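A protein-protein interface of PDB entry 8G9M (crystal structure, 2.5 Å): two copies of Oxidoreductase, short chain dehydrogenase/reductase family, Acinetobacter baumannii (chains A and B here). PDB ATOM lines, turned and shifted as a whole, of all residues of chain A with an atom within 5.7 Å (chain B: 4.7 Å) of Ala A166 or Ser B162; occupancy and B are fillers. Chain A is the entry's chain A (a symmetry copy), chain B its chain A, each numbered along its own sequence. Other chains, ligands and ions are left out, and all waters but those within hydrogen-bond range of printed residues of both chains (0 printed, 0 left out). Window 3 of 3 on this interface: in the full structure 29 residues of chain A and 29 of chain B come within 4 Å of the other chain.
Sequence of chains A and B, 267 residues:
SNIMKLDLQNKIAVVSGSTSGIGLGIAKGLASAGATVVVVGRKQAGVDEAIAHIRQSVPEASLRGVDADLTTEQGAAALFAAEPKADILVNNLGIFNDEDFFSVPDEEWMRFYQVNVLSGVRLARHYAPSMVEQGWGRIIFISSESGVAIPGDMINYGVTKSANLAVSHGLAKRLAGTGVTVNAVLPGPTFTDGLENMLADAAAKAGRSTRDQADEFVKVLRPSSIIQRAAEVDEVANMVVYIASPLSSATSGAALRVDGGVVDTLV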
ATOM      1  N   LYS A 161      -4.685  15.234   3.016  1.00  0.00           N
ATOM      2  CA  LYS A 161      -4.607  15.963   4.280  1.00  0.00           C
ATOM      3  C   LYS A 161      -5.947  16.601   4.642  1.00  0.00           C
ATOM      4  O   LYS A 161      -6.405  16.506   5.791  1.00  0.00           O
ATOM      5  CB  LYS A 161      -3.499  17.013   4.204  1.00  0.00           C
ATOM      6  N   SER A 162      -6.597  17.251   3.672  1.00  0.00           N
ATOM      7  CA  SER A 162      -7.927  17.804   3.925  1.00  0.00           C
ATOM      8  C   SER A 162      -8.959  16.704   4.157  1.00  0.00           C
ATOM      9  O   SER A 162      -9.919  16.900   4.917  1.00  0.00           O
ATOM     10  CB  SER A 162      -8.356  18.699   2.766  1.00  0.00           C
ATOM     11  OG  SER A 162      -7.854  18.208   1.539  1.00  0.00           O
ATOM     12  N   ALA A 163      -8.773  15.538   3.532  1.00  0.00           N
ATOM     13  CA  ALA A 163      -9.632  14.399   3.837  1.00  0.00           C
ATOM     14  C   ALA A 163      -9.493  13.980   5.295  1.00  0.00           C
ATOM     15  O   ALA A 163     -10.485  13.645   5.951  1.00  0.00           O
ATOM     16  CB  ALA A 163      -9.302  13.235   2.909  1.00  0.00           C
ATOM     17  N   ASN A 164      -8.263  13.985   5.818  1.00  0.00           N
ATOM     18  CA  ASN A 164      -8.048  13.664   7.228  1.00  0.00           C
ATOM     19  C   ASN A 164      -8.697  14.703   8.134  1.00  0.00           C
ATOM     20  O   ASN A 164      -9.281  14.360   9.172  1.00  0.00           O
ATOM     21  CB  ASN A 164      -6.551  13.567   7.525  1.00  0.00           C
ATOM     22  CG  ASN A 164      -5.957  12.246   7.091  1.00  0.00           C
ATOM     23  OD1 ASN A 164      -6.656  11.237   7.015  1.00  0.00           O
ATOM     24  ND2 ASN A 164      -4.660  12.240   6.808  1.00  0.00           N
ATOM     25  N   LEU A 165      -8.572  15.983   7.772  1.00  0.00           N
ATOM     26  CA  LEU A 165      -9.252  17.030   8.530  1.00  0.00           C
ATOM     27  C   LEU A 165     -10.754  16.775   8.576  1.00  0.00           C
ATOM     28  O   LEU A 165     -11.387  16.885   9.637  1.00  0.00           O
ATOM     29  CB  LEU A 165      -8.955  18.399   7.921  1.00  0.00           C
ATOM     30  CG  LEU A 165      -7.500  18.865   8.009  1.00  0.00           C
ATOM     31  CD1 LEU A 165      -7.224  19.991   7.025  1.00  0.00           C
ATOM     32  CD2 LEU A 165      -7.161  19.294   9.427  1.00  0.00           C
ATOM     33  N   ALA A 166     -11.336  16.420   7.427  1.00  0.00           N
ATOM     34  CA  ALA A 166     -12.750  16.073   7.372  1.00  0.00           C
ATOM     35  C   ALA A 166     -13.066  14.874   8.256  1.00  0.00           C
ATOM     36  O   ALA A 166     -14.095  14.852   8.941  1.00  0.00           O
ATOM     37  CB  ALA A 166     -13.152  15.786   5.926  1.00  0.00           C
ATOM     38  N   VAL A 167     -12.201  13.858   8.233  1.00  0.00           N
ATOM     39  CA  VAL A 167     -12.417  12.663   9.046  1.00  0.00           C
ATOM     40  C   VAL A 167     -12.493  13.036  10.520  1.00  0.00           C
ATOM     41  O   VAL A 167     -13.396  12.600  11.248  1.00  0.00           O
ATOM     42  CB  VAL A 167     -11.302  11.632   8.791  1.00  0.00           C
ATOM     43  CG1 VAL A 167     -11.273  10.604   9.909  1.00  0.00           C
ATOM     44  CG2 VAL A 167     -11.486  10.946   7.450  1.00  0.00           C
ATOM     45  N   SER A 168     -11.546  13.857  10.977  1.00  0.00           N
ATOM     46  CA  SER A 168     -11.504  14.206  12.395  1.00  0.00           C
ATOM     47  C   SER A 168     -12.704  15.067  12.782  1.00  0.00           C
ATOM     48  O   SER A 168     -13.313  14.853  13.834  1.00  0.00           O
ATOM     49  CB  SER A 168     -10.206  14.932  12.734  1.00  0.00           C
ATOM     50  OG  SER A 168     -10.392  16.334  12.794  1.00  0.00           O
ATOM     51  N   HIS A 169     -13.074  16.032  11.935  1.00  0.00           N
ATOM     52  CA  HIS A 169     -14.255  16.850  12.205  1.00  0.00           C
ATOM     53  C   HIS A 169     -15.512  15.988  12.313  1.00  0.00           C
ATOM     54  O   HIS A 169     -16.289  16.100  13.277  1.00  0.00           O
ATOM     55  CB  HIS A 169     -14.396  17.894  11.100  1.00  0.00           C
ATOM     56  CG  HIS A 169     -15.232  19.074  11.482  1.00  0.00           C
ATOM     57  ND1 HIS A 169     -16.545  18.964  11.888  1.00  0.00           N
ATOM     58  CD2 HIS A 169     -14.945  20.397  11.498  1.00  0.00           C
ATOM     59  CE1 HIS A 169     -17.029  20.168  12.144  1.00  0.00           C
ATOM     60  NE2 HIS A 169     -16.077  21.054  11.915  1.00  0.00           N
ATOM     61  N   GLY A 170     -15.722  15.110  11.331  1.00  0.00           N
ATOM     62  CA  GLY A 170     -16.923  14.295  11.318  1.00  0.00           C
ATOM     63  C   GLY A 170     -16.983  13.307  12.466  1.00  0.00           C
ATOM     64  O   GLY A 170     -18.035  13.131  13.086  1.00  0.00           O
ATOM     65  N   LEU A 171     -15.863  12.643  12.769  1.00  0.00           N
ATOM     66  CA  LEU A 171     -15.880  11.700  13.880  1.00  0.00           C
ATOM     67  C   LEU A 171     -15.996  12.426  15.213  1.00  0.00           C
ATOM     68  O   LEU A 171     -16.545  11.868  16.169  1.00  0.00           O
ATOM     69  CB  LEU A 171     -14.641  10.807  13.863  1.00  0.00           C
ATOM     70  CG  LEU A 171     -14.742   9.586  14.787  1.00  0.00           C
ATOM     71  CD1 LEU A 171     -16.133   8.968  14.721  1.00  0.00           C
ATOM     72  CD2 LEU A 171     -13.684   8.550  14.453  1.00  0.00           C
ATOM     73  N   GLY B 147     -19.363  19.461   2.628  1.00  0.00           N
ATOM     74  CA  GLY B 147     -17.925  19.348   2.465  1.00  0.00           C
ATOM     75  C   GLY B 147     -17.127  20.257   3.371  1.00  0.00           C
ATOM     76  O   GLY B 147     -15.979  19.944   3.703  1.00  0.00           O
ATOM     77  N   ILE B 150     -18.307  18.640   8.033  1.00  0.00           N
ATOM     78  CA  ILE B 150     -18.646  17.223   7.863  1.00  0.00           C
ATOM     79  C   ILE B 150     -19.731  16.842   8.863  1.00  0.00           C
ATOM     80  O   ILE B 150     -19.555  17.056  10.078  1.00  0.00           O
ATOM     81  CB  ILE B 150     -17.395  16.346   8.044  1.00  0.00           C
ATOM     82  CG1 ILE B 150     -16.242  16.848   7.165  1.00  0.00           C
ATOM     83  CG2 ILE B 150     -17.708  14.896   7.710  1.00  0.00           C
ATOM     84  CD1 ILE B 150     -16.628  17.284   5.756  1.00  0.00           C
ATOM     85  N   GLY B 158     -19.000  13.408   3.362  1.00  0.00           N
ATOM     86  CA  GLY B 158     -18.390  14.700   3.633  1.00  0.00           C
ATOM     87  C   GLY B 158     -16.898  14.704   3.358  1.00  0.00           C
ATOM     88  O   GLY B 158     -16.344  15.694   2.866  1.00  0.00           O
ATOM     89  N   VAL B 159     -16.227  13.592   3.672  1.00  0.00           N
ATOM     90  CA  VAL B 159     -14.806  13.463   3.364  1.00  0.00           C
ATOM     91  C   VAL B 159     -14.580  13.579   1.862  1.00  0.00           C
ATOM     92  O   VAL B 159     -13.675  14.287   1.407  1.00  0.00           O
ATOM     93  CB  VAL B 159     -14.253  12.139   3.919  1.00  0.00           C
ATOM     94  CG1 VAL B 159     -12.906  11.814   3.287  1.00  0.00           C
ATOM     95  CG2 VAL B 159     -14.125  12.216   5.427  1.00  0.00           C
ATOM     96  N   THR B 160     -15.409  12.892   1.068  1.00  0.00           N
ATOM     97  CA  THR B 160     -15.250  12.979  -0.384  1.00  0.00           C
ATOM     98  C   THR B 160     -15.540  14.389  -0.896  1.00  0.00           C
ATOM     99  O   THR B 160     -14.876  14.871  -1.824  1.00  0.00           O
ATOM    100  CB  THR B 160     -16.147  11.959  -1.091  1.00  0.00           C
ATOM    101  OG1 THR B 160     -17.524  12.309  -0.903  1.00  0.00           O
ATOM    102  CG2 THR B 160     -15.889  10.553  -0.567  1.00  0.00           C
ATOM    103  N   LYS B 161     -16.516  15.072  -0.295  1.00  0.00           N
ATOM    104  CA  LYS B 161     -16.851  16.422  -0.744  1.00  0.00           C
ATOM    105  C   LYS B 161     -15.712  17.401  -0.470  1.00  0.00           C
ATOM    106  O   LYS B 161     -15.340  18.202  -1.342  1.00  0.00           O
ATOM    107  CB  LYS B 161     -18.146  16.882  -0.074  1.00  0.00           C
ATOM    108  N   SER B 162     -15.135  17.349   0.735  1.00  0.00           N
ATOM    109  CA  SER B 162     -13.978  18.192   1.030  1.00  0.00           C
ATOM    110  C   SER B 162     -12.759  17.785   0.206  1.00  0.00           C
ATOM    111  O   SER B 162     -11.928  18.638  -0.142  1.00  0.00           O
ATOM    112  CB  SER B 162     -13.653  18.141   2.521  1.00  0.00           C
ATOM    113  OG  SER B 162     -13.936  16.862   3.052  1.00  0.00           O
ATOM    114  N   ALA B 163     -12.642  16.499  -0.132  1.00  0.00           N
ATOM    115  CA  ALA B 163     -11.590  16.076  -1.050  1.00  0.00           C
ATOM    116  C   ALA B 163     -11.759  16.728  -2.416  1.00  0.00           C
ATOM    117  O   ALA B 163     -10.775  17.140  -3.042  1.00  0.00           O
ATOM    118  CB  ALA B 163     -11.589  14.557  -1.176  1.00  0.00           C
ATOM    119  N   ASN B 164     -13.001  16.823  -2.900  1.00  0.00           N
ATOM    120  CA  ASN B 164     -13.259  17.496  -4.172  1.00  0.00           C
ATOM    121  C   ASN B 164     -12.922  18.980  -4.087  1.00  0.00           C
ATOM    122  O   ASN B 164     -12.366  19.557  -5.033  1.00  0.00           O
ATOM    123  CB  ASN B 164     -14.721  17.310  -4.580  1.00  0.00           C
ATOM    124  CG  ASN B 164     -14.984  15.955  -5.197  1.00  0.00           C
ATOM    125  OD1 ASN B 164     -14.083  15.335  -5.760  1.00  0.00           O
ATOM    126  ND2 ASN B 164     -16.222  15.487  -5.100  1.00  0.00           N
ATOM    127  N   LEU B 165     -13.284  19.619  -2.972  1.00  0.00           N
ATOM    128  CA  LEU B 165     -12.906  21.016  -2.771  1.00  0.00           C
ATOM    129  C   LEU B 165     -11.393  21.183  -2.850  1.00  0.00           C
ATOM    130  O   LEU B 165     -10.888  22.107  -3.505  1.00  0.00           O
ATOM    131  CB  LEU B 165     -13.434  21.516  -1.427  1.00  0.00           C
ATOM    132  CG  LEU B 165     -14.957  21.599  -1.300  1.00  0.00           C
ATOM    133  CD1 LEU B 165     -15.382  21.679   0.158  1.00  0.00           C
ATOM    134  CD2 LEU B 165     -15.495  22.783  -2.084  1.00  0.00           C
ATOM    135  N   ALA B 166     -10.656  20.282  -2.195  1.00  0.00           N
ATOM    136  CA  ALA B 166      -9.200  20.297  -2.270  1.00  0.00           C
ATOM    137  C   ALA B 166      -8.713  20.107  -3.700  1.00  0.00           C
ATOM    138  O   ALA B 166      -7.763  20.769  -4.133  1.00  0.00           O
ATOM    139  CB  ALA B 166      -8.629  19.208  -1.364  1.00  0.00           C
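The backbone carbonyl oxygen (O) of Gly B158 is in hydrogen-bond range of the side-chain hydroxyl (OG) of Ser B162 (2.7 Å). The backbone carbonyl oxygen (O) of Val B159 sits at hydrogen-bond distance from the side-chain hydroxyl (OG) of Ser B162, 3.1 Å away.
Among the printed residues, merely in contact across the chains: Ser A162 with Ala B166 (3.2 Å), Ala A166 with Ser B162 (3.2 Å), Ala A166 with Ile B150 (3.4 Å), Val A167 with Val B159 (3.6 Å), Ala A166 with Val B159 (3.7 Å), Gly A170 with Ile B150 (3.7 Å), Ala A163 with Val B159 (3.9 Å) and His A169 with Ile B150 (3.997 Å).
Of the printed residues of chain B, Ala A166 touches Ile B150, Val B159 and Ser B162. Ser B162 touches just one residue of chain A: Ala A166 (3.2 Å). Of the printed residues of chain B, Val A167 touches Val B159 (3.6 Å). Of the printed residues of chain B, Ser A162 touches Ala B166 (3.2 Å). Ser A168 touches none of the printed residues of chain B. Thr B160 touches none of the printed residues of chain A. The nearest residue of chain A that does not touch Ser B162 is Ser A162 (4.4 Å).
Of the 11 printed residues of chain B, 4 touch a printed residue of chain A. Along chain B the printed residues that touch a printed residue of chain A span positions 150 to 166. Hydrophobic or aromatic side chains of chain A that line the printed part of chain B: Ala A163, Ala A166, Val A167 and His A169. Among the printed residues, no Asp or Glu carboxylate lies within 4 Å of a Lys or Arg side-chain nitrogen of the other chain.
Ser A162 touches Ala B166, and with the chains exchanged Ala A166 touches Ser B162.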
